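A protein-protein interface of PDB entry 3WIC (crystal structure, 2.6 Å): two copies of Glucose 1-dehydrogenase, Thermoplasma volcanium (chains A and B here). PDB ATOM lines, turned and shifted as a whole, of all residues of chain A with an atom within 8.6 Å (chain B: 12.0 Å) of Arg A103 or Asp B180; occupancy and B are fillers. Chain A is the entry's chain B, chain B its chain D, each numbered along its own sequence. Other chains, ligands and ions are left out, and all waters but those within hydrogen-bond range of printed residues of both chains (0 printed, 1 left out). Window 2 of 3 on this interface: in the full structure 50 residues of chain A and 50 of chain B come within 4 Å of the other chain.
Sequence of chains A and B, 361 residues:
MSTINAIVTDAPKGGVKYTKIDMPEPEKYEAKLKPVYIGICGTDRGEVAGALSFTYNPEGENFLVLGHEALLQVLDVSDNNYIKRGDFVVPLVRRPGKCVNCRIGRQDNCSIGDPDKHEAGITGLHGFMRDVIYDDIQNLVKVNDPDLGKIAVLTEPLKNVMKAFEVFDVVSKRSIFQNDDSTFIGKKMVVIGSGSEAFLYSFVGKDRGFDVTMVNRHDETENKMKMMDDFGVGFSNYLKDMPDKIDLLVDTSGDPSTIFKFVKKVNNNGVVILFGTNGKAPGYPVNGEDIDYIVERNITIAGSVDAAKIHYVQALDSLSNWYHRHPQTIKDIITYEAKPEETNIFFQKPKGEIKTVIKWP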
ATOM      1  N   ARG A  95     -28.729  11.937 -19.795  1.00  0.00           N
ATOM      2  CA  ARG A  95     -29.463  11.367 -20.904  1.00  0.00           C
ATOM      3  C   ARG A  95     -28.941   9.964 -21.212  1.00  0.00           C
ATOM      4  O   ARG A  95     -27.752   9.733 -21.120  1.00  0.00           O
ATOM      5  CB  ARG A  95     -29.362  12.298 -22.150  1.00  0.00           C
ATOM      6  CG  ARG A  95     -29.773  13.743 -21.885  1.00  0.00           C
ATOM      7  CD  ARG A  95     -31.138  13.832 -21.201  1.00  0.00           C
ATOM      8  NE  ARG A  95     -31.537  15.179 -20.734  1.00  0.00           N
ATOM      9  CZ  ARG A  95     -32.131  16.129 -21.473  1.00  0.00           C
ATOM     10  NH1 ARG A  95     -32.374  15.947 -22.772  1.00  0.00           N
ATOM     11  NH2 ARG A  95     -32.473  17.278 -20.908  1.00  0.00           N
ATOM     12  N   PRO A  96     -29.837   9.038 -21.612  1.00  0.00           N
ATOM     13  CA  PRO A  96     -29.472   7.626 -21.850  1.00  0.00           C
ATOM     14  C   PRO A  96     -28.588   7.394 -23.055  1.00  0.00           C
ATOM     15  O   PRO A  96     -28.744   8.065 -24.048  1.00  0.00           O
ATOM     16  CB  PRO A  96     -30.831   6.956 -22.120  1.00  0.00           C
ATOM     17  CG  PRO A  96     -31.696   8.033 -22.656  1.00  0.00           C
ATOM     18  CD  PRO A  96     -31.257   9.295 -21.934  1.00  0.00           C
ATOM     19  N   GLY A  97     -27.694   6.419 -22.967  1.00  0.00           N
ATOM     20  CA  GLY A  97     -27.088   5.804 -24.155  1.00  0.00           C
ATOM     21  C   GLY A  97     -27.814   4.530 -24.590  1.00  0.00           C
ATOM     22  O   GLY A  97     -29.035   4.507 -24.678  1.00  0.00           O
ATOM     23  N   LYS A  98     -27.041   3.475 -24.862  1.00  0.00           N
ATOM     24  CA  LYS A  98     -27.544   2.220 -25.413  1.00  0.00           C
ATOM     25  C   LYS A  98     -27.271   0.971 -24.560  1.00  0.00           C
ATOM     26  O   LYS A  98     -27.633  -0.125 -24.969  1.00  0.00           O
ATOM     27  CB  LYS A  98     -26.945   2.026 -26.801  1.00  0.00           C
ATOM     28  CG  LYS A  98     -27.596   2.899 -27.863  1.00  0.00           C
ATOM     29  CD  LYS A  98     -26.939   2.711 -29.231  1.00  0.00           C
ATOM     30  CE  LYS A  98     -27.607   3.527 -30.342  1.00  0.00           C
ATOM     31  NZ  LYS A  98     -29.034   3.137 -30.599  1.00  0.00           N
ATOM     32  N   CYS A  99     -26.647   1.126 -23.391  1.00  0.00           N
ATOM     33  CA  CYS A  99     -26.355  -0.031 -22.519  1.00  0.00           C
ATOM     34  C   CYS A  99     -27.633  -0.547 -21.812  1.00  0.00           C
ATOM     35  O   CYS A  99     -28.572   0.211 -21.596  1.00  0.00           O
ATOM     36  CB  CYS A  99     -25.265   0.283 -21.479  1.00  0.00           C
ATOM     37  SG  CYS A  99     -25.871   1.120 -20.021  1.00  0.00           S
ATOM     38  N   VAL A 100     -27.617  -1.831 -21.454  1.00  0.00           N
ATOM     39  CA  VAL A 100     -28.738  -2.548 -20.815  1.00  0.00           C
ATOM     40  C   VAL A 100     -29.466  -1.747 -19.757  1.00  0.00           C
ATOM     41  O   VAL A 100     -30.671  -1.928 -19.605  1.00  0.00           O
ATOM     42  CB  VAL A 100     -28.335  -3.944 -20.207  1.00  0.00           C
ATOM     43  CG1 VAL A 100     -27.494  -3.819 -18.944  1.00  0.00           C
ATOM     44  CG2 VAL A 100     -29.564  -4.782 -19.890  1.00  0.00           C
ATOM     45  N   ASN A 101     -28.730  -0.911 -19.010  1.00  0.00           N
ATOM     46  CA  ASN A 101     -29.313   0.014 -18.026  1.00  0.00           C
ATOM     47  C   ASN A 101     -29.846   1.292 -18.686  1.00  0.00           C
ATOM     48  O   ASN A 101     -30.947   1.735 -18.358  1.00  0.00           O
ATOM     49  CB  ASN A 101     -28.320   0.372 -16.897  1.00  0.00           C
ATOM     50  CG  ASN A 101     -28.232  -0.703 -15.817  1.00  0.00           C
ATOM     51  OD1 ASN A 101     -29.092  -0.795 -14.946  1.00  0.00           O
ATOM     52  ND2 ASN A 101     -27.194  -1.526 -15.883  1.00  0.00           N
ATOM     53  N   CYS A 102     -29.094   1.872 -19.618  1.00  0.00           N
ATOM     54  CA  CYS A 102     -29.566   3.065 -20.305  1.00  0.00           C
ATOM     55  C   CYS A 102     -30.873   2.833 -21.063  1.00  0.00           C
ATOM     56  O   CYS A 102     -31.748   3.702 -21.019  1.00  0.00           O
ATOM     57  CB  CYS A 102     -28.495   3.661 -21.236  1.00  0.00           C
ATOM     58  SG  CYS A 102     -27.237   4.639 -20.349  1.00  0.00           S
ATOM     59  N   ARG A 103     -31.033   1.679 -21.718  1.00  0.00           N
ATOM     60  CA  ARG A 103     -32.244   1.467 -22.529  1.00  0.00           C
ATOM     61  C   ARG A 103     -33.579   1.259 -21.742  1.00  0.00           C
ATOM     62  O   ARG A 103     -34.666   1.114 -22.352  1.00  0.00           O
ATOM     63  CB  ARG A 103     -32.042   0.360 -23.553  1.00  0.00           C
ATOM     64  CG  ARG A 103     -32.147  -1.079 -23.072  1.00  0.00           C
ATOM     65  CD  ARG A 103     -30.834  -1.730 -23.270  1.00  0.00           C
ATOM     66  NE  ARG A 103     -30.833  -2.913 -24.102  1.00  0.00           N
ATOM     67  CZ  ARG A 103     -29.726  -3.373 -24.691  1.00  0.00           C
ATOM     68  NH1 ARG A 103     -28.575  -2.728 -24.548  1.00  0.00           N
ATOM     69  NH2 ARG A 103     -29.759  -4.474 -25.419  1.00  0.00           N
ATOM     70  N   ILE A 104     -33.491   1.238 -20.403  1.00  0.00           N
ATOM     71  CA  ILE A 104     -34.681   1.063 -19.561  1.00  0.00           C
ATOM     72  C   ILE A 104     -34.932   2.251 -18.616  1.00  0.00           C
ATOM     73  O   ILE A 104     -35.686   2.134 -17.646  1.00  0.00           O
ATOM     74  CB  ILE A 104     -34.670  -0.289 -18.807  1.00  0.00           C
ATOM     75  CG1 ILE A 104     -33.472  -0.399 -17.878  1.00  0.00           C
ATOM     76  CG2 ILE A 104     -34.659  -1.465 -19.797  1.00  0.00           C
ATOM     77  CD1 ILE A 104     -33.843  -1.030 -16.537  1.00  0.00           C
ATOM     78  N   GLY A 105     -34.316   3.397 -18.920  1.00  0.00           N
ATOM     79  CA  GLY A 105     -34.488   4.601 -18.131  1.00  0.00           C
ATOM     80  C   GLY A 105     -33.606   4.632 -16.884  1.00  0.00           C
ATOM     81  O   GLY A 105     -33.906   5.381 -15.907  1.00  0.00           O
ATOM     82  N   ARG A 106     -32.526   3.832 -16.889  1.00  0.00           N
ATOM     83  CA  ARG A 106     -31.566   3.849 -15.746  1.00  0.00           C
ATOM     84  C   ARG A 106     -30.147   4.215 -16.180  1.00  0.00           C
ATOM     85  O   ARG A 106     -29.181   3.542 -15.855  1.00  0.00           O
ATOM     86  CB  ARG A 106     -31.599   2.537 -14.937  1.00  0.00           C
ATOM     87  CG  ARG A 106     -32.986   2.173 -14.413  1.00  0.00           C
ATOM     88  CD  ARG A 106     -33.574   3.200 -13.450  1.00  0.00           C
ATOM     89  NE  ARG A 106     -32.662   3.446 -12.344  1.00  0.00           N
ATOM     90  CZ  ARG A 106     -32.877   3.209 -11.043  1.00  0.00           C
ATOM     91  NH1 ARG A 106     -34.028   2.734 -10.577  1.00  0.00           N
ATOM     92  NH2 ARG A 106     -31.915   3.472 -10.172  1.00  0.00           N
ATOM     93  N   GLN A 107     -30.047   5.315 -16.911  1.00  0.00           N
ATOM     94  CA  GLN A 107     -28.763   5.867 -17.321  1.00  0.00           C
ATOM     95  C   GLN A 107     -27.884   6.266 -16.099  1.00  0.00           C
ATOM     96  O   GLN A 107     -26.635   6.403 -16.191  1.00  0.00           O
ATOM     97  CB  GLN A 107     -28.994   7.056 -18.286  1.00  0.00           C
ATOM     98  CG  GLN A 107     -29.913   8.195 -17.831  1.00  0.00           C
ATOM     99  CD  GLN A 107     -31.388   7.993 -18.249  1.00  0.00           C
ATOM    100  OE1 GLN A 107     -31.865   6.868 -18.354  1.00  0.00           O
ATOM    101  NE2 GLN A 107     -32.109   9.091 -18.473  1.00  0.00           N
ATOM    102  N   ASN A 109     -27.384   4.408 -13.704  1.00  0.00           N
ATOM    103  CA  ASN A 109     -26.657   3.178 -13.466  1.00  0.00           C
ATOM    104  C   ASN A 109     -26.009   2.576 -14.755  1.00  0.00           C
ATOM    105  O   ASN A 109     -25.964   1.357 -14.946  1.00  0.00           O
ATOM    106  CB  ASN A 109     -27.622   2.175 -12.819  1.00  0.00           C
ATOM    107  CG  ASN A 109     -27.997   2.563 -11.407  1.00  0.00           C
ATOM    108  OD1 ASN A 109     -27.211   3.182 -10.694  1.00  0.00           O
ATOM    109  ND2 ASN A 109     -29.203   2.172 -10.979  1.00  0.00           N
ATOM    110  N   CYS A 110     -25.512   3.446 -15.620  1.00  0.00           N
ATOM    111  CA  CYS A 110     -24.888   3.061 -16.881  1.00  0.00           C
ATOM    112  C   CYS A 110     -23.737   2.112 -16.614  1.00  0.00           C
ATOM    113  O   CYS A 110     -23.004   2.347 -15.659  1.00  0.00           O
ATOM    114  CB  CYS A 110     -24.340   4.324 -17.566  1.00  0.00           C
ATOM    115  SG  CYS A 110     -23.763   4.091 -19.257  1.00  0.00           S
ATOM    116  N   SER A 111     -23.603   1.081 -17.462  1.00  0.00           N
ATOM    117  CA  SER A 111     -22.606   0.017 -17.342  1.00  0.00           C
ATOM    118  C   SER A 111     -21.345   0.294 -18.148  1.00  0.00           C
ATOM    119  O   SER A 111     -20.440  -0.529 -18.198  1.00  0.00           O
ATOM    120  CB  SER A 111     -23.136  -1.320 -17.892  1.00  0.00           C
ATOM    121  OG  SER A 111     -24.488  -1.525 -17.569  1.00  0.00           O
ATOM    122  N   ILE A 112     -21.321   1.403 -18.855  1.00  0.00           N
ATOM    123  CA  ILE A 112     -20.137   1.763 -19.605  1.00  0.00           C
ATOM    124  C   ILE A 112     -19.499   3.015 -19.000  1.00  0.00           C
ATOM    125  O   ILE A 112     -18.287   3.051 -18.775  1.00  0.00           O
ATOM    126  CB  ILE A 112     -20.505   1.949 -21.067  1.00  0.00           C
ATOM    127  CG1 ILE A 112     -20.995   0.614 -21.626  1.00  0.00           C
ATOM    128  CG2 ILE A 112     -19.320   2.506 -21.848  1.00  0.00           C
ATOM    129  CD1 ILE A 112     -21.633   0.722 -22.998  1.00  0.00           C
ATOM    130  N   ASP A 116     -21.265   6.582 -23.366  1.00  0.00           N
ATOM    131  CA  ASP A 116     -22.589   6.016 -23.612  1.00  0.00           C
ATOM    132  C   ASP A 116     -23.647   7.049 -23.216  1.00  0.00           C
ATOM    133  O   ASP A 116     -24.411   7.494 -24.059  1.00  0.00           O
ATOM    134  CB  ASP A 116     -22.788   4.698 -22.873  1.00  0.00           C
ATOM    135  CG  ASP A 116     -23.834   3.809 -23.539  1.00  0.00           C
ATOM    136  OD1 ASP A 116     -24.004   3.890 -24.781  1.00  0.00           O
ATOM    137  OD2 ASP A 116     -24.494   3.024 -22.817  1.00  0.00           O
ATOM    138  N   GLN A 138     -40.097  13.522 -23.098  1.00  0.00           N
ATOM    139  CA  GLN A 138     -39.655  12.427 -22.238  1.00  0.00           C
ATOM    140  C   GLN A 138     -38.623  12.846 -21.197  1.00  0.00           C
ATOM    141  O   GLN A 138     -38.437  12.161 -20.177  1.00  0.00           O
ATOM    142  CB  GLN A 138     -39.079  11.287 -23.095  1.00  0.00           C
ATOM    143  CG  GLN A 138     -40.118  10.380 -23.741  1.00  0.00           C
ATOM    144  CD  GLN A 138     -40.126   8.952 -23.193  1.00  0.00           C
ATOM    145  OE1 GLN A 138     -39.069   8.399 -22.909  1.00  0.00           O
ATOM    146  NE2 GLN A 138     -41.316   8.337 -23.083  1.00  0.00           N
ATOM    147  N   SER B 175     -28.886  -2.491  -9.798  1.00  0.00           N
ATOM    148  CA  SER B 175     -28.898  -2.142 -11.184  1.00  0.00           C
ATOM    149  C   SER B 175     -29.017  -3.443 -11.905  1.00  0.00           C
ATOM    150  O   SER B 175     -29.134  -4.472 -11.287  1.00  0.00           O
ATOM    151  CB  SER B 175     -27.622  -1.341 -11.560  1.00  0.00           C
ATOM    152  OG  SER B 175     -26.433  -2.116 -11.414  1.00  0.00           O
ATOM    153  N   ILE B 176     -28.970  -3.415 -13.215  1.00  0.00           N
ATOM    154  CA  ILE B 176     -28.916  -4.659 -13.943  1.00  0.00           C
ATOM    155  C   ILE B 176     -27.473  -4.978 -14.272  1.00  0.00           C
ATOM    156  O   ILE B 176     -26.868  -4.343 -15.124  1.00  0.00           O
ATOM    157  CB  ILE B 176     -29.756  -4.638 -15.230  1.00  0.00           C
ATOM    158  CG1 ILE B 176     -31.237  -4.513 -14.833  1.00  0.00           C
ATOM    159  CG2 ILE B 176     -29.494  -5.891 -16.071  1.00  0.00           C
ATOM    160  CD1 ILE B 176     -32.073  -4.040 -16.004  1.00  0.00           C
ATOM    161  N   PHE B 177     -27.011  -6.056 -13.626  1.00  0.00           N
ATOM    162  CA  PHE B 177     -25.629  -6.504 -13.600  1.00  0.00           C
ATOM    163  C   PHE B 177     -25.289  -7.388 -14.775  1.00  0.00           C
ATOM    164  O   PHE B 177     -24.126  -7.460 -15.214  1.00  0.00           O
ATOM    165  CB  PHE B 177     -25.426  -7.305 -12.286  1.00  0.00           C
ATOM    166  CG  PHE B 177     -23.989  -7.499 -11.920  1.00  0.00           C
ATOM    167  CD1 PHE B 177     -23.282  -8.606 -12.391  1.00  0.00           C
ATOM    168  CD2 PHE B 177     -23.346  -6.577 -11.101  1.00  0.00           C
ATOM    169  CE1 PHE B 177     -21.956  -8.771 -12.077  1.00  0.00           C
ATOM    170  CE2 PHE B 177     -22.018  -6.755 -10.768  1.00  0.00           C
ATOM    171  CZ  PHE B 177     -21.322  -7.849 -11.258  1.00  0.00           C
ATOM    172  N   GLN B 178     -26.311  -8.143 -15.185  1.00  0.00           N
ATOM    173  CA  GLN B 178     -26.188  -9.174 -16.199  1.00  0.00           C
ATOM    174  C   GLN B 178     -25.982  -8.504 -17.538  1.00  0.00           C
ATOM    175  O   GLN B 178     -26.088  -7.284 -17.674  1.00  0.00           O
ATOM    176  CB  GLN B 178     -27.455 -10.018 -16.269  1.00  0.00           C
ATOM    177  CG  GLN B 178     -27.784 -10.776 -15.009  1.00  0.00           C
ATOM    178  CD  GLN B 178     -28.447  -9.963 -13.900  1.00  0.00           C
ATOM    179  OE1 GLN B 178     -28.978  -8.849 -14.098  1.00  0.00           O
ATOM    180  NE2 GLN B 178     -28.424 -10.537 -12.701  1.00  0.00           N
ATOM    181  N   ASN B 179     -25.674  -9.301 -18.534  1.00  0.00           N
ATOM    182  CA  ASN B 179     -25.737  -8.798 -19.882  1.00  0.00           C
ATOM    183  C   ASN B 179     -27.211  -8.563 -20.270  1.00  0.00           C
ATOM    184  O   ASN B 179     -28.150  -8.951 -19.532  1.00  0.00           O
ATOM    185  CB  ASN B 179     -25.134  -9.829 -20.842  1.00  0.00           C
ATOM    186  CG  ASN B 179     -23.706 -10.133 -20.521  1.00  0.00           C
ATOM    187  OD1 ASN B 179     -22.897  -9.216 -20.286  1.00  0.00           O
ATOM    188  ND2 ASN B 179     -23.378 -11.414 -20.470  1.00  0.00           N
ATOM    189  N   ASP B 180     -27.391  -8.017 -21.477  1.00  0.00           N
ATOM    190  CA  ASP B 180     -28.697  -7.865 -22.089  1.00  0.00           C
ATOM    191  C   ASP B 180     -29.247  -9.166 -22.670  1.00  0.00           C
ATOM    192  O   ASP B 180     -30.206  -9.131 -23.422  1.00  0.00           O
ATOM    193  CB  ASP B 180     -28.664  -6.765 -23.155  1.00  0.00           C
ATOM    194  CG  ASP B 180     -27.778  -7.093 -24.332  1.00  0.00           C
ATOM    195  OD1 ASP B 180     -27.224  -8.205 -24.456  1.00  0.00           O
ATOM    196  OD2 ASP B 180     -27.618  -6.190 -25.144  1.00  0.00           O
ATOM    197  N   ASP B 181     -28.692 -10.303 -22.285  1.00  0.00           N
ATOM    198  CA  ASP B 181     -29.300 -11.617 -22.519  1.00  0.00           C
ATOM    199  C   ASP B 181     -29.723 -12.365 -21.266  1.00  0.00           C
ATOM    200  O   ASP B 181     -30.200 -13.465 -21.320  1.00  0.00           O
ATOM    201  CB  ASP B 181     -28.437 -12.499 -23.447  1.00  0.00           C
ATOM    202  CG  ASP B 181     -27.066 -12.810 -22.896  1.00  0.00           C
ATOM    203  OD1 ASP B 181     -26.724 -12.367 -21.820  1.00  0.00           O
ATOM    204  OD2 ASP B 181     -26.319 -13.508 -23.566  1.00  0.00           O
ATOM    205  N   SER B 182     -29.542 -11.717 -20.137  1.00  0.00           N
ATOM    206  CA  SER B 182     -29.886 -12.199 -18.811  1.00  0.00           C
ATOM    207  C   SER B 182     -28.838 -12.956 -18.065  1.00  0.00           C
ATOM    208  O   SER B 182     -29.038 -13.261 -16.927  1.00  0.00           O
ATOM    209  CB  SER B 182     -31.146 -13.018 -18.811  1.00  0.00           C
ATOM    210  OG  SER B 182     -31.059 -14.086 -19.670  1.00  0.00           O
ATOM    211  N   THR B 183     -27.709 -13.223 -18.699  1.00  0.00           N
ATOM    212  CA  THR B 183     -26.652 -14.072 -18.163  1.00  0.00           C
ATOM    213  C   THR B 183     -25.485 -13.293 -17.664  1.00  0.00           C
ATOM    214  O   THR B 183     -25.403 -12.113 -17.826  1.00  0.00           O
ATOM    215  CB  THR B 183     -26.110 -15.092 -19.169  1.00  0.00           C
ATOM    216  OG1 THR B 183     -25.312 -14.421 -20.114  1.00  0.00           O
ATOM    217  CG2 THR B 183     -27.189 -15.776 -19.897  1.00  0.00           C
ATOM    218  N   PHE B 184     -24.588 -14.004 -17.032  1.00  0.00           N
ATOM    219  CA  PHE B 184     -23.386 -13.446 -16.447  1.00  0.00           C
ATOM    220  C   PHE B 184     -22.206 -13.799 -17.357  1.00  0.00           C
ATOM    221  O   PHE B 184     -21.061 -13.728 -16.957  1.00  0.00           O
ATOM    222  CB  PHE B 184     -23.142 -14.067 -15.070  1.00  0.00           C
ATOM    223  CG  PHE B 184     -24.098 -13.635 -14.024  1.00  0.00           C
ATOM    224  CD1 PHE B 184     -25.292 -14.321 -13.822  1.00  0.00           C
ATOM    225  CD2 PHE B 184     -23.794 -12.585 -13.180  1.00  0.00           C
ATOM    226  CE1 PHE B 184     -26.181 -13.932 -12.837  1.00  0.00           C
ATOM    227  CE2 PHE B 184     -24.677 -12.204 -12.188  1.00  0.00           C
ATOM    228  CZ  PHE B 184     -25.866 -12.884 -12.021  1.00  0.00           C
ATOM    229  N   ILE B 185     -22.473 -14.208 -18.577  1.00  0.00           N
ATOM    230  CA  ILE B 185     -21.386 -14.711 -19.457  1.00  0.00           C
ATOM    231  C   ILE B 185     -20.442 -13.561 -19.801  1.00  0.00           C
ATOM    232  O   ILE B 185     -20.889 -12.490 -20.224  1.00  0.00           O
ATOM    233  CB  ILE B 185     -21.951 -15.321 -20.744  1.00  0.00           C
ATOM    234  CG1 ILE B 185     -22.774 -16.570 -20.443  1.00  0.00           C
ATOM    235  CG2 ILE B 185     -20.861 -15.669 -21.724  1.00  0.00           C
ATOM    236  CD1 ILE B 185     -23.773 -16.875 -21.547  1.00  0.00           C
ATOM    237  N   GLY B 186     -19.147 -13.783 -19.581  1.00  0.00           N
ATOM    238  CA  GLY B 186     -18.103 -12.793 -19.883  1.00  0.00           C
ATOM    239  C   GLY B 186     -17.868 -11.779 -18.777  1.00  0.00           C
ATOM    240  O   GLY B 186     -16.975 -10.929 -18.879  1.00  0.00           O
ATOM    241  N   LYS B 187     -18.685 -11.870 -17.728  1.00  0.00           N
ATOM    242  CA  LYS B 187     -18.603 -11.002 -16.591  1.00  0.00           C
ATOM    243  C   LYS B 187     -17.432 -11.494 -15.821  1.00  0.00           C
ATOM    244  O   LYS B 187     -17.379 -12.701 -15.495  1.00  0.00           O
ATOM    245  CB  LYS B 187     -19.825 -11.134 -15.679  1.00  0.00           C
ATOM    246  CG  LYS B 187     -21.072 -10.440 -16.196  1.00  0.00           C
ATOM    247  CD  LYS B 187     -20.987  -8.924 -16.123  1.00  0.00           C
ATOM    248  CE  LYS B 187     -21.983  -8.320 -17.114  1.00  0.00           C
ATOM    249  NZ  LYS B 187     -21.903  -6.821 -17.165  1.00  0.00           N
ATOM    250  N   ASP B 247     -15.840  -7.165 -12.853  1.00  0.00           N
ATOM    251  CA  ASP B 247     -17.229  -6.970 -12.415  1.00  0.00           C
ATOM    252  C   ASP B 247     -17.523  -7.387 -10.958  1.00  0.00           C
ATOM    253  O   ASP B 247     -18.321  -6.725 -10.268  1.00  0.00           O
ATOM    254  CB  ASP B 247     -18.120  -7.710 -13.349  1.00  0.00           C
ATOM    255  CG  ASP B 247     -18.019  -7.183 -14.691  1.00  0.00           C
ATOM    256  OD1 ASP B 247     -18.421  -6.011 -14.784  1.00  0.00           O
ATOM    257  OD2 ASP B 247     -17.520  -7.885 -15.596  1.00  0.00           O
ATOM    258  N   ASN B 269     -20.966  -0.408 -11.794  1.00  0.00           N
ATOM    259  CA  ASN B 269     -21.933  -1.328 -11.164  1.00  0.00           C
ATOM    260  C   ASN B 269     -21.248  -2.477 -10.556  1.00  0.00           C
ATOM    261  O   ASN B 269     -21.897  -3.469 -10.216  1.00  0.00           O
ATOM    262  CB  ASN B 269     -23.019  -1.776 -12.158  1.00  0.00           C
ATOM    263  CG  ASN B 269     -23.834  -0.596 -12.652  1.00  0.00           C
ATOM    264  OD1 ASN B 269     -24.196   0.268 -11.863  1.00  0.00           O
ATOM    265  ND2 ASN B 269     -24.063  -0.513 -13.946  1.00  0.00           N
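The backbone carbonyl oxygen of Cys A110 sits at hydrogen-bond distance from the side-chain amide nitrogen of Asn B269 (3.5 Å).
NH2 of Arg A103 is in salt-bridge range of OD2 of Asp B180 (2.8 Å).
The backbone carbonyl oxygen (O) of Asn A109 lies within hydrogen-bond range of the side-chain amide nitrogen (ND2) of Asn B269 (2.8 Å).
O of Ile B176 sits at hydrogen-bond distance from ND2 of Asn A101 (2.9 Å).
NH1 of Arg A103 sits at hydrogen-bond distance from O of Lys A98, at 2.8 Å.
O of Asn A109 lies close to ND2 of Asn A101 (3.3 Å).
The side-chain sulfur (SG) of Cys A99 lies close to the backbone NH (N) of Ser A111, 3.4 Å away.
The side-chain amide nitrogen (ND2) of Asn A101 is in hydrogen-bond range of the side-chain hydroxyl (OG) of Ser A111 (3.2 Å).
The backbone NH of Ile A112 sits close to the side-chain sulfur of Cys A110.
The guanidinium group (NH2) of Arg A106 lies close to the side-chain amide nitrogen (ND2) of Asn A109, at 3.1 Å.
Among the printed residues, pairs that only touch across the chains: Ile A104 with Ile B176, Asn A101 with Ser B175, Ser A111 with Asn B269, Asn A109 with Ser B175, Asn A101 with Asn B269, Val A100 with Asp B180, Val A100 with Ile B176 and Val A100 with Gln B178.
Arg A103 touches just one residue of chain B: Asp B180 (2.8 Å).
Of chain A, only Val A100 (3.9 Å) and Arg A103 (2.8 Å) come within 4 Å of Asp B180.
Pro A96 touches none of the printed residues of chain B.
No residue of chain B comes within 4 Å of Gly A97.
No residue of chain B comes within 4 Å of Cys A99.
Of the printed residues of chain B, Val A100 touches Ile B176 (3.9 Å), Gln B178 (3.9 Å) and Asp B180 (3.9 Å).
Of chain B, only Ser B175 (3.7 Å), Ile B176 (2.9 Å) and Asn B269 (3.8 Å) come within 4 Å of Asn A101.
No residue of chain B comes within 4 Å of Cys A102.
Ile A104 touches one residue of chain B.
Gly A105 touches none of the printed residues of chain B.
Of the printed residues of chain B, Asn A109 touches Ser B175 and Asn B269.
Of the printed residues of chain B, Ser A111 touches Asn B269.
Of the printed residues of chain A, Ile B176 touches Val A100 (3.9 Å), Asn A101 (2.9 Å) and Ile A104 (3.5 Å).
Thr B183 touches none of the printed residues of chain A.
The nearest printed residue of chain B that does not touch Cys A110 is Ser B175 (6.6 Å).
Of the 15 printed residues of chain B, 5 touch a printed residue of chain A.
Hydrophobic or aromatic side chains of chain B that line the printed part of chain A: Ile B176.
Among the printed residues, 12 pairs touch across the chains.
Among the printed residues, Asp or Glu carboxylates within 4 Å of a Lys or Arg side-chain nitrogen of the other chain: Arg A103 with Asp B180 (2.8 Å).
No position is printed for both chains.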
